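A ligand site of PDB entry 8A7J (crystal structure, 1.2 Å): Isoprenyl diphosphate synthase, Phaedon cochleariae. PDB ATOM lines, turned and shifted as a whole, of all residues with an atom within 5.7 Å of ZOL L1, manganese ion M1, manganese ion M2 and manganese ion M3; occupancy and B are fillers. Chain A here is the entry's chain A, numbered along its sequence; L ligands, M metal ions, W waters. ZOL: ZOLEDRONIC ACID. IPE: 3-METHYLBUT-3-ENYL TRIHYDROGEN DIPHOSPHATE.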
ATOM      1  N   LEU A  92      30.628 -15.450  25.310  1.00  0.00           N
ATOM      2  CA  LEU A  92      30.391 -16.644  24.469  1.00  0.00           C
ATOM      3  C   LEU A  92      29.448 -17.633  25.158  1.00  0.00           C
ATOM      4  O   LEU A  92      28.582 -18.207  24.511  1.00  0.00           O
ATOM      5  CB  LEU A  92      31.743 -17.286  24.131  1.00  0.00           C
ATOM      6  CG  LEU A  92      32.615 -16.470  23.185  1.00  0.00           C
ATOM      7  CD1 LEU A  92      34.028 -17.028  23.155  1.00  0.00           C
ATOM      8  CD2 LEU A  92      32.023 -16.442  21.808  1.00  0.00           C
ATOM      9  N   LEU A  93      29.623 -17.855  26.460  1.00  0.00           N
ATOM     10  CA  LEU A  93      28.798 -18.845  27.167  1.00  0.00           C
ATOM     11  C   LEU A  93      27.345 -18.371  27.267  1.00  0.00           C
ATOM     12  O   LEU A  93      26.436 -19.203  27.162  1.00  0.00           O
ATOM     13  CB  LEU A  93      29.356 -19.226  28.530  1.00  0.00           C
ATOM     14  CG  LEU A  93      30.799 -19.779  28.507  1.00  0.00           C
ATOM     15  CD1 LEU A  93      31.157 -20.278  29.918  1.00  0.00           C
ATOM     16  CD2 LEU A  93      30.949 -20.911  27.493  1.00  0.00           C
ATOM     17  N   ASP A  96      26.006 -19.101  23.871  1.00  0.00           N
ATOM     18  CA  ASP A  96      26.059 -20.532  23.598  1.00  0.00           C
ATOM     19  C   ASP A  96      24.920 -21.266  24.318  1.00  0.00           C
ATOM     20  O   ASP A  96      24.322 -22.167  23.723  1.00  0.00           O
ATOM     21  CB  ASP A  96      27.431 -21.059  23.988  1.00  0.00           C
ATOM     22  CG  ASP A  96      27.547 -22.554  23.715  1.00  0.00           C
ATOM     23  OD1 ASP A  96      27.839 -22.898  22.533  1.00  0.00           O
ATOM     24  OD2 ASP A  96      27.352 -23.340  24.699  1.00  0.00           O
ATOM     25  N   ASP A  97      24.657 -20.899  25.560  1.00  0.00           N
ATOM     26  CA  ASP A  97      23.595 -21.567  26.328  1.00  0.00           C
ATOM     27  C   ASP A  97      22.215 -21.301  25.701  1.00  0.00           C
ATOM     28  O   ASP A  97      21.395 -22.219  25.694  1.00  0.00           O
ATOM     29  CB  ASP A  97      23.664 -21.131  27.787  1.00  0.00           C
ATOM     30  CG  ASP A  97      24.836 -21.771  28.521  1.00  0.00           C
ATOM     31  OD1 ASP A  97      25.272 -22.863  28.081  1.00  0.00           O
ATOM     32  OD2 ASP A  97      25.219 -21.235  29.569  1.00  0.00           O
ATOM     33  N   ASP A 100      22.171 -23.563  22.520  1.00  0.00           N
ATOM     34  CA  ASP A 100      22.188 -25.002  22.828  1.00  0.00           C
ATOM     35  C   ASP A 100      21.023 -25.381  23.746  1.00  0.00           C
ATOM     36  O   ASP A 100      20.886 -26.573  24.059  1.00  0.00           O
ATOM     37  CB  ASP A 100      23.550 -25.381  23.439  1.00  0.00           C
ATOM     38  CG  ASP A 100      24.675 -25.188  22.454  1.00  0.00           C
ATOM     39  OD1 ASP A 100      24.392 -25.059  21.268  1.00  0.00           O
ATOM     40  OD2 ASP A 100      25.881 -25.187  22.908  1.00  0.00           O
ATOM     41  N   SER A 102      20.443 -24.902  26.779  1.00  0.00           N
ATOM     42  CA  SER A 102      20.996 -25.535  27.978  1.00  0.00           C
ATOM     43  C   SER A 102      20.240 -25.136  29.250  1.00  0.00           C
ATOM     44  O   SER A 102      19.499 -24.144  29.283  1.00  0.00           O
ATOM     45  CB  SER A 102      22.465 -25.227  28.088  1.00  0.00           C
ATOM     46  OG  SER A 102      23.199 -25.859  27.039  1.00  0.00           O
ATOM     47  N   ARG A 105      24.619 -23.691  33.905  1.00  0.00           N
ATOM     48  CA  ARG A 105      25.996 -23.236  33.585  1.00  0.00           C
ATOM     49  C   ARG A 105      26.655 -22.893  34.919  1.00  0.00           C
ATOM     50  O   ARG A 105      26.090 -22.136  35.693  1.00  0.00           O
ATOM     51  CB  ARG A 105      25.936 -22.002  32.681  1.00  0.00           C
ATOM     52  CG  ARG A 105      27.272 -21.332  32.462  1.00  0.00           C
ATOM     53  CD  ARG A 105      28.307 -22.144  31.687  1.00  0.00           C
ATOM     54  NE  ARG A 105      27.875 -22.347  30.322  1.00  0.00           N
ATOM     55  CZ  ARG A 105      28.535 -23.071  29.428  1.00  0.00           C
ATOM     56  NH1 ARG A 105      29.659 -23.664  29.744  1.00  0.00           N
ATOM     57  NH2 ARG A 105      28.081 -23.180  28.181  1.00  0.00           N
ATOM     58  N   THR A 160      36.103 -17.260  16.179  1.00  0.00           N
ATOM     59  CA  THR A 160      35.223 -17.990  17.112  1.00  0.00           C
ATOM     60  C   THR A 160      33.806 -18.010  16.585  1.00  0.00           C
ATOM     61  O   THR A 160      33.137 -19.059  16.616  1.00  0.00           O
ATOM     62  CB  THR A 160      35.298 -17.424  18.530  1.00  0.00           C
ATOM     63  OG1 THR A 160      36.670 -17.380  18.989  1.00  0.00           O
ATOM     64  CG2 THR A 160      34.496 -18.219  19.516  1.00  0.00           C
ATOM     65  N   GLN A 164      31.511 -21.298  15.795  1.00  0.00           N
ATOM     66  CA  GLN A 164      30.181 -21.438  16.400  1.00  0.00           C
ATOM     67  C   GLN A 164      29.154 -21.697  15.283  1.00  0.00           C
ATOM     68  O   GLN A 164      28.238 -22.471  15.457  1.00  0.00           O
ATOM     69  CB  GLN A 164      29.849 -20.217  17.217  1.00  0.00           C
ATOM     70  CG  GLN A 164      28.635 -20.329  18.069  1.00  0.00           C
ATOM     71  CD  GLN A 164      28.817 -21.172  19.312  1.00  0.00           C
ATOM     72  OE1 GLN A 164      29.885 -21.851  19.498  1.00  0.00           O
ATOM     73  NE2 GLN A 164      27.787 -21.107  20.149  1.00  0.00           N
ATOM     74  N   ASP A 167      29.730 -25.346  13.992  1.00  0.00           N
ATOM     75  CA  ASP A 167      29.165 -26.207  15.050  1.00  0.00           C
ATOM     76  C   ASP A 167      27.634 -26.303  14.886  1.00  0.00           C
ATOM     77  O   ASP A 167      27.066 -27.406  15.048  1.00  0.00           O
ATOM     78  CB  ASP A 167      29.532 -25.643  16.408  1.00  0.00           C
ATOM     79  CG  ASP A 167      29.002 -26.420  17.589  1.00  0.00           C
ATOM     80  OD1 ASP A 167      27.851 -26.127  17.963  1.00  0.00           O
ATOM     81  OD2 ASP A 167      29.748 -27.256  18.115  1.00  0.00           O
ATOM     82  N   LYS A 193      35.947 -22.874  17.032  1.00  0.00           N
ATOM     83  CA  LYS A 193      35.009 -22.515  18.112  1.00  0.00           C
ATOM     84  C   LYS A 193      35.666 -22.484  19.478  1.00  0.00           C
ATOM     85  O   LYS A 193      35.062 -21.926  20.405  1.00  0.00           O
ATOM     86  CB  LYS A 193      33.766 -23.420  18.141  1.00  0.00           C
ATOM     87  CG  LYS A 193      33.964 -24.783  18.793  1.00  0.00           C
ATOM     88  CD  LYS A 193      32.684 -25.466  19.129  1.00  0.00           C
ATOM     89  CE  LYS A 193      32.922 -26.830  19.738  1.00  0.00           C
ATOM     90  NZ  LYS A 193      31.651 -27.488  20.163  1.00  0.00           N
ATOM     91  N   THR A 194      36.834 -23.092  19.630  1.00  0.00           N
ATOM     92  CA  THR A 194      37.455 -23.283  20.956  1.00  0.00           C
ATOM     93  C   THR A 194      38.938 -22.912  20.978  1.00  0.00           C
ATOM     94  O   THR A 194      39.368 -22.165  21.878  1.00  0.00           O
ATOM     95  CB  THR A 194      37.239 -24.698  21.488  1.00  0.00           C
ATOM     96  OG1 THR A 194      35.865 -24.763  21.845  1.00  0.00           O
ATOM     97  CG2 THR A 194      38.126 -25.002  22.664  1.00  0.00           C
ATOM     98  N   TYR A 197      40.385 -19.010  21.014  1.00  0.00           N
ATOM     99  CA  TYR A 197      40.114 -18.098  22.132  1.00  0.00           C
ATOM    100  C   TYR A 197      40.565 -18.711  23.456  1.00  0.00           C
ATOM    101  O   TYR A 197      40.842 -17.972  24.399  1.00  0.00           O
ATOM    102  CB  TYR A 197      38.657 -17.654  22.197  1.00  0.00           C
ATOM    103  CG  TYR A 197      37.719 -18.531  23.006  1.00  0.00           C
ATOM    104  CD1 TYR A 197      37.019 -19.597  22.447  1.00  0.00           C
ATOM    105  CD2 TYR A 197      37.460 -18.254  24.329  1.00  0.00           C
ATOM    106  CE1 TYR A 197      36.135 -20.362  23.184  1.00  0.00           C
ATOM    107  CE2 TYR A 197      36.568 -18.994  25.080  1.00  0.00           C
ATOM    108  CZ  TYR A 197      35.897 -20.055  24.505  1.00  0.00           C
ATOM    109  OH  TYR A 197      35.004 -20.803  25.207  1.00  0.00           O
ATOM    110  N   GLN A 233      38.712 -29.794  23.881  1.00  0.00           N
ATOM    111  CA  GLN A 233      37.320 -29.906  23.406  1.00  0.00           C
ATOM    112  C   GLN A 233      36.850 -31.351  23.406  1.00  0.00           C
ATOM    113  O   GLN A 233      35.649 -31.584  23.666  1.00  0.00           O
ATOM    114  CB  GLN A 233      37.146 -29.209  22.069  1.00  0.00           C
ATOM    115  CG  GLN A 233      35.687 -29.103  21.656  1.00  0.00           C
ATOM    116  CD  GLN A 233      34.858 -28.270  22.585  1.00  0.00           C
ATOM    117  OE1 GLN A 233      35.238 -27.148  22.939  1.00  0.00           O
ATOM    118  NE2 GLN A 233      33.695 -28.784  22.974  1.00  0.00           N
ATOM    119  N   ASP A 236      35.740 -31.923  26.765  1.00  0.00           N
ATOM    120  CA  ASP A 236      34.444 -31.251  26.990  1.00  0.00           C
ATOM    121  C   ASP A 236      33.316 -32.131  26.450  1.00  0.00           C
ATOM    122  O   ASP A 236      32.243 -32.241  27.090  1.00  0.00           O
ATOM    123  CB  ASP A 236      34.411 -29.881  26.325  1.00  0.00           C
ATOM    124  CG  ASP A 236      33.120 -29.147  26.613  1.00  0.00           C
ATOM    125  OD1 ASP A 236      32.921 -28.825  27.820  1.00  0.00           O
ATOM    126  OD2 ASP A 236      32.336 -28.917  25.650  1.00  0.00           O
ATOM    127  N   ASP A 237      33.524 -32.671  25.262  1.00  0.00           N
ATOM    128  CA  ASP A 237      32.489 -33.501  24.634  1.00  0.00           C
ATOM    129  C   ASP A 237      32.238 -34.764  25.473  1.00  0.00           C
ATOM    130  O   ASP A 237      31.083 -35.201  25.614  1.00  0.00           O
ATOM    131  CB  ASP A 237      32.915 -33.859  23.222  1.00  0.00           C
ATOM    132  CG  ASP A 237      32.972 -32.709  22.250  1.00  0.00           C
ATOM    133  OD1 ASP A 237      32.611 -31.572  22.626  1.00  0.00           O
ATOM    134  OD2 ASP A 237      33.436 -32.955  21.108  1.00  0.00           O
ATOM    135  N   ASP A 240      30.023 -33.865  28.352  1.00  0.00           N
ATOM    136  CA  ASP A 240      28.599 -33.586  28.024  1.00  0.00           C
ATOM    137  C   ASP A 240      27.749 -34.833  28.286  1.00  0.00           C
ATOM    138  O   ASP A 240      26.644 -34.698  28.868  1.00  0.00           O
ATOM    139  CB  ASP A 240      28.476 -33.137  26.569  1.00  0.00           C
ATOM    140  CG  ASP A 240      27.090 -32.657  26.215  1.00  0.00           C
ATOM    141  OD1 ASP A 240      26.811 -31.454  26.422  1.00  0.00           O
ATOM    142  OD2 ASP A 240      26.304 -33.486  25.801  1.00  0.00           O
ATOM    143  N   LYS A 250      27.117 -28.180  34.538  1.00  0.00           N
ATOM    144  CA  LYS A 250      26.278 -28.029  33.346  1.00  0.00           C
ATOM    145  C   LYS A 250      25.703 -29.373  32.954  1.00  0.00           C
ATOM    146  O   LYS A 250      26.352 -30.411  33.045  1.00  0.00           O
ATOM    147  CB  LYS A 250      27.079 -27.359  32.222  1.00  0.00           C
ATOM    148  CG  LYS A 250      28.260 -28.134  31.714  1.00  0.00           C
ATOM    149  CD  LYS A 250      29.195 -27.269  30.820  1.00  0.00           C
ATOM    150  CE  LYS A 250      30.207 -28.123  30.110  1.00  0.00           C
ATOM    151  NZ  LYS A 250      31.166 -27.305  29.336  1.00  0.00           N
ATOM    152  N   THR A 253      23.770 -31.431  26.464  1.00  0.00           N
ATOM    153  CA  THR A 253      22.729 -31.273  25.413  1.00  0.00           C
ATOM    154  C   THR A 253      23.204 -31.770  24.047  1.00  0.00           C
ATOM    155  O   THR A 253      22.463 -31.606  23.076  1.00  0.00           O
ATOM    156  CB  THR A 253      22.335 -29.803  25.264  1.00  0.00           C
ATOM    157  OG1 THR A 253      23.505 -29.030  24.962  1.00  0.00           O
ATOM    158  CG2 THR A 253      21.616 -29.302  26.496  1.00  0.00           C
ATOM    159  N   ASP A 254      24.420 -32.305  23.894  1.00  0.00           N
ATOM    160  CA  ASP A 254      24.926 -32.539  22.533  1.00  0.00           C
ATOM    161  C   ASP A 254      24.101 -33.566  21.750  1.00  0.00           C
ATOM    162  O   ASP A 254      23.900 -33.402  20.540  1.00  0.00           O
ATOM    163  CB  ASP A 254      26.391 -32.959  22.535  1.00  0.00           C
ATOM    164  CG  ASP A 254      27.390 -31.906  22.949  1.00  0.00           C
ATOM    165  OD1 ASP A 254      27.052 -30.689  22.883  1.00  0.00           O
ATOM    166  OD2 ASP A 254      28.538 -32.308  23.294  1.00  0.00           O
ATOM    167  N   LYS A 259      24.716 -32.696  17.755  1.00  0.00           N
ATOM    168  CA  LYS A 259      26.049 -32.120  17.514  1.00  0.00           C
ATOM    169  C   LYS A 259      27.048 -33.126  16.950  1.00  0.00           C
ATOM    170  O   LYS A 259      27.017 -34.317  17.273  1.00  0.00           O
ATOM    171  CB  LYS A 259      26.581 -31.559  18.811  1.00  0.00           C
ATOM    172  CG  LYS A 259      25.838 -30.346  19.323  1.00  0.00           C
ATOM    173  CD  LYS A 259      26.066 -29.110  18.477  1.00  0.00           C
ATOM    174  CE  LYS A 259      25.004 -28.067  18.530  1.00  0.00           C
ATOM    175  NZ  LYS A 259      24.835 -27.598  19.913  1.00  0.00           N
HETATM  176  O17 ZOL L   1      30.810 -25.960  22.206  1.00  0.00           O
HETATM  177  P14 ZOL L   1      29.981 -26.326  23.425  1.00  0.00           P
HETATM  178  O16 ZOL L   1      28.534 -25.753  23.344  1.00  0.00           O
HETATM  179  O15 ZOL L   1      29.998 -27.831  23.724  1.00  0.00           O
HETATM  180  C8  ZOL L   1      30.710 -25.541  24.929  1.00  0.00           C
HETATM  181  P9  ZOL L   1      29.777 -25.965  26.461  1.00  0.00           P
HETATM  182  O10 ZOL L   1      29.922 -27.477  26.625  1.00  0.00           O
HETATM  183  O11 ZOL L   1      28.361 -25.549  26.254  1.00  0.00           O
HETATM  184  O12 ZOL L   1      30.464 -25.210  27.588  1.00  0.00           O
HETATM  185  O13 ZOL L   1      32.059 -26.053  25.084  1.00  0.00           O
HETATM  186  C7  ZOL L   1      30.828 -24.020  24.799  1.00  0.00           C
HETATM  187  N15 ZOL L   1      31.667 -23.563  23.677  1.00  0.00           N
HETATM  188  C16 ZOL L   1      32.949 -23.910  23.406  1.00  0.00           C
HETATM  189  N17 ZOL L   1      33.371 -23.293  22.333  1.00  0.00           N
HETATM  190  C18 ZOL L   1      32.363 -22.506  21.890  1.00  0.00           C
HETATM  191  C19 ZOL L   1      31.319 -22.624  22.734  1.00  0.00           C
HETATM  192  C1  IPE L   2      33.806 -24.167  28.526  1.00  0.00           C
HETATM  193  O1  IPE L   2      35.105 -23.786  29.061  1.00  0.00           O
HETATM  194  C2  IPE L   2      33.806 -23.979  27.032  1.00  0.00           C
HETATM  195  C3  IPE L   2      34.865 -24.760  26.277  1.00  0.00           C
HETATM  196  C4  IPE L   2      35.614 -24.172  25.364  1.00  0.00           C
HETATM  197  C5  IPE L   2      34.933 -26.192  26.599  1.00  0.00           C
HETATM  198  PA  IPE L   2      35.531 -24.184  30.538  1.00  0.00           P
HETATM  199  O1A IPE L   2      35.269 -25.626  30.773  1.00  0.00           O
HETATM  200  O2A IPE L   2      36.934 -23.691  30.705  1.00  0.00           O
HETATM  201  O3A IPE L   2      34.504 -23.375  31.410  1.00  0.00           O
HETATM  202  PB  IPE L   2      34.610 -22.265  32.638  1.00  0.00           P
HETATM  203  O1B IPE L   2      33.247 -22.327  33.277  1.00  0.00           O
HETATM  204  O2B IPE L   2      35.706 -22.755  33.552  1.00  0.00           O
HETATM  205  O3B IPE L   2      34.915 -20.951  32.014  1.00  0.00           O
HETATM  206 MN    MN M   1      27.006 -25.347  24.742  1.00  0.00          MN
HETATM  207 MN    MN M   2      27.626 -24.793  21.659  1.00  0.00          MN
HETATM  208 MN    MN M   3      30.216 -29.037  25.397  1.00  0.00          MN
HETATM  209  O   HOH W   1      30.174 -30.306  27.134  1.00  0.00           O
HETATM  210  O   HOH W   2      26.432 -23.835  20.220  1.00  0.00           O
HETATM  211  O   HOH W   3      30.514 -30.705  24.195  1.00  0.00           O
HETATM  212  O   HOH W   4      27.493 -26.650  20.626  1.00  0.00           O
HETATM  213  O   HOH W   5      28.730 -28.924  21.599  1.00  0.00           O
HETATM  214  O   HOH W   6      25.495 -24.793  26.048  1.00  0.00           O
HETATM  215  O   HOH W   7      26.880 -27.046  28.185  1.00  0.00           O
HETATM  216  O   HOH W   8      29.384 -24.430  20.584  1.00  0.00           O
HETATM  217  O   HOH W   9      28.106 -29.508  25.190  1.00  0.00           O
HETATM  218  O   HOH W  10      26.369 -27.336  24.794  1.00  0.00           O
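Within 4 Å of manganese ion M3: Asp 236.
Two residues have an atom within 4 Å of manganese ion M1: Asp 96 and Asp 100. The nearest printed residue that does not touch manganese ion M1 is Arg 105 (4.2 Å).
OG1 of Thr 194 lies within hydrogen-bond range of N17 of ZOL L1, 2.9 Å away. The side-chain amino group (NZ) of Lys 250 lies within salt-bridge range of an oxygen (O12) of ZOL L1 (2.8 Å). The guanidinium group of Arg 105 lies within salt-bridge range of an oxygen (O12) of ZOL L1 (2.8 Å). NZ of Lys 193 lies within salt-bridge range of O17 of ZOL L1 (2.7 Å).
Manganese ion M3 is bound by an oxygen (O10) of ZOL L1 (2.0 Å), an oxygen (O15) of ZOL L1 (2.1 Å), water W3 (2.1 Å), the side-chain carboxylate (OD2) of Asp 236 (2.1 Å), water W1 (2.2 Å) and water W9 (2.2 Å).
Gln 164 touches manganese ion M2. Asp 167 touches manganese ion M2. Four residues have an atom within 4 Å of manganese ion M2: Asp 96, Asp 100, Gln 164 and Asp 167. The nearest printed residue that does not touch manganese ion M2 is Lys 259 (4.3 Å).
Manganese ion M1 is bound by the side-chain carboxylate of Asp 96, an oxygen (O11) of ZOL L1, water W6, water W10, an oxygen (O16) of ZOL L1 and the side-chain carboxylate of Asp 100.
Manganese ion M2 is bound by water W8 (2.1 Å). Manganese ion M2 is bound by OD1 of Asp 96 (2.1 Å). Water W2 is bound to manganese ion M2, at 2.1 Å. Manganese ion M2 is bound by water W4. Manganese ion M2 is bound by O16 of ZOL L1, at 2.1 Å. OD2 of Asp 100 binds manganese ion M2 (2.2 Å). Manganese ion M2 has six donor atoms within binding distance.
Residues that only touch ZOL L1: Gln 164 and Gln 233. The nearest printed residue that does not touch ZOL L1 is Leu 93 (4.1 Å).
The side-chain carboxylate of Asp 236 sits close to the side-chain amide nitrogen of Gln 233. The side-chain carboxylate of Asp 96 sits close to the guanidinium group of Arg 105, at 3.6 Å. The side-chain amide nitrogen of Gln 233 lies within hydrogen-bond range of the side-chain carboxylate of Asp 237, at 3.0 Å. The side-chain carboxylate (OD1) of Asp 96 lies close to the side-chain amide nitrogen (NE2) of Gln 164. The side-chain carboxylate (OD2) of Asp 167 is in salt-bridge range of the side-chain amino group (NZ) of Lys 193. OD1 of Asp 97 lies within salt-bridge range of NH2 of Arg 105 (2.8 Å). The side-chain amino group (NZ) of Lys 250 is in salt-bridge range of the side-chain carboxylate (OD1) of Asp 236, at 2.8 Å. NZ of Lys 259 lies within salt-bridge range of OD1 of Asp 100.
Water W6 lies within hydrogen-bond range of the side-chain hydroxyl (OG) of Ser 102 (2.7 Å) and the side-chain carboxylate (OD1) of Asp 97 (2.8 Å). Water W8 lies within hydrogen-bond range of an oxygen (O17) of ZOL L1 (2.6 Å), the side-chain amide oxygen (OE1) of Gln 164 (2.8 Å) and the side-chain carboxylate (OD1) of Asp 167 (3.5 Å). Water W2 lies within hydrogen-bond range of OD1 of Asp 100 and NE2 of Gln 164. Water W4 bridges OD1 of Asp 167 (2.7 Å) and NZ of Lys 259 (2.9 Å). Water W9 bridges the side-chain carboxylate (OD1) of Asp 240 (2.6 Å) and the side-chain carboxylate (OD1) of Asp 254 (2.8 Å). Water W3 bridges the side-chain carboxylate of Asp 254 (2.7 Å) and the side-chain carboxylate of Asp 237 (2.8 Å).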
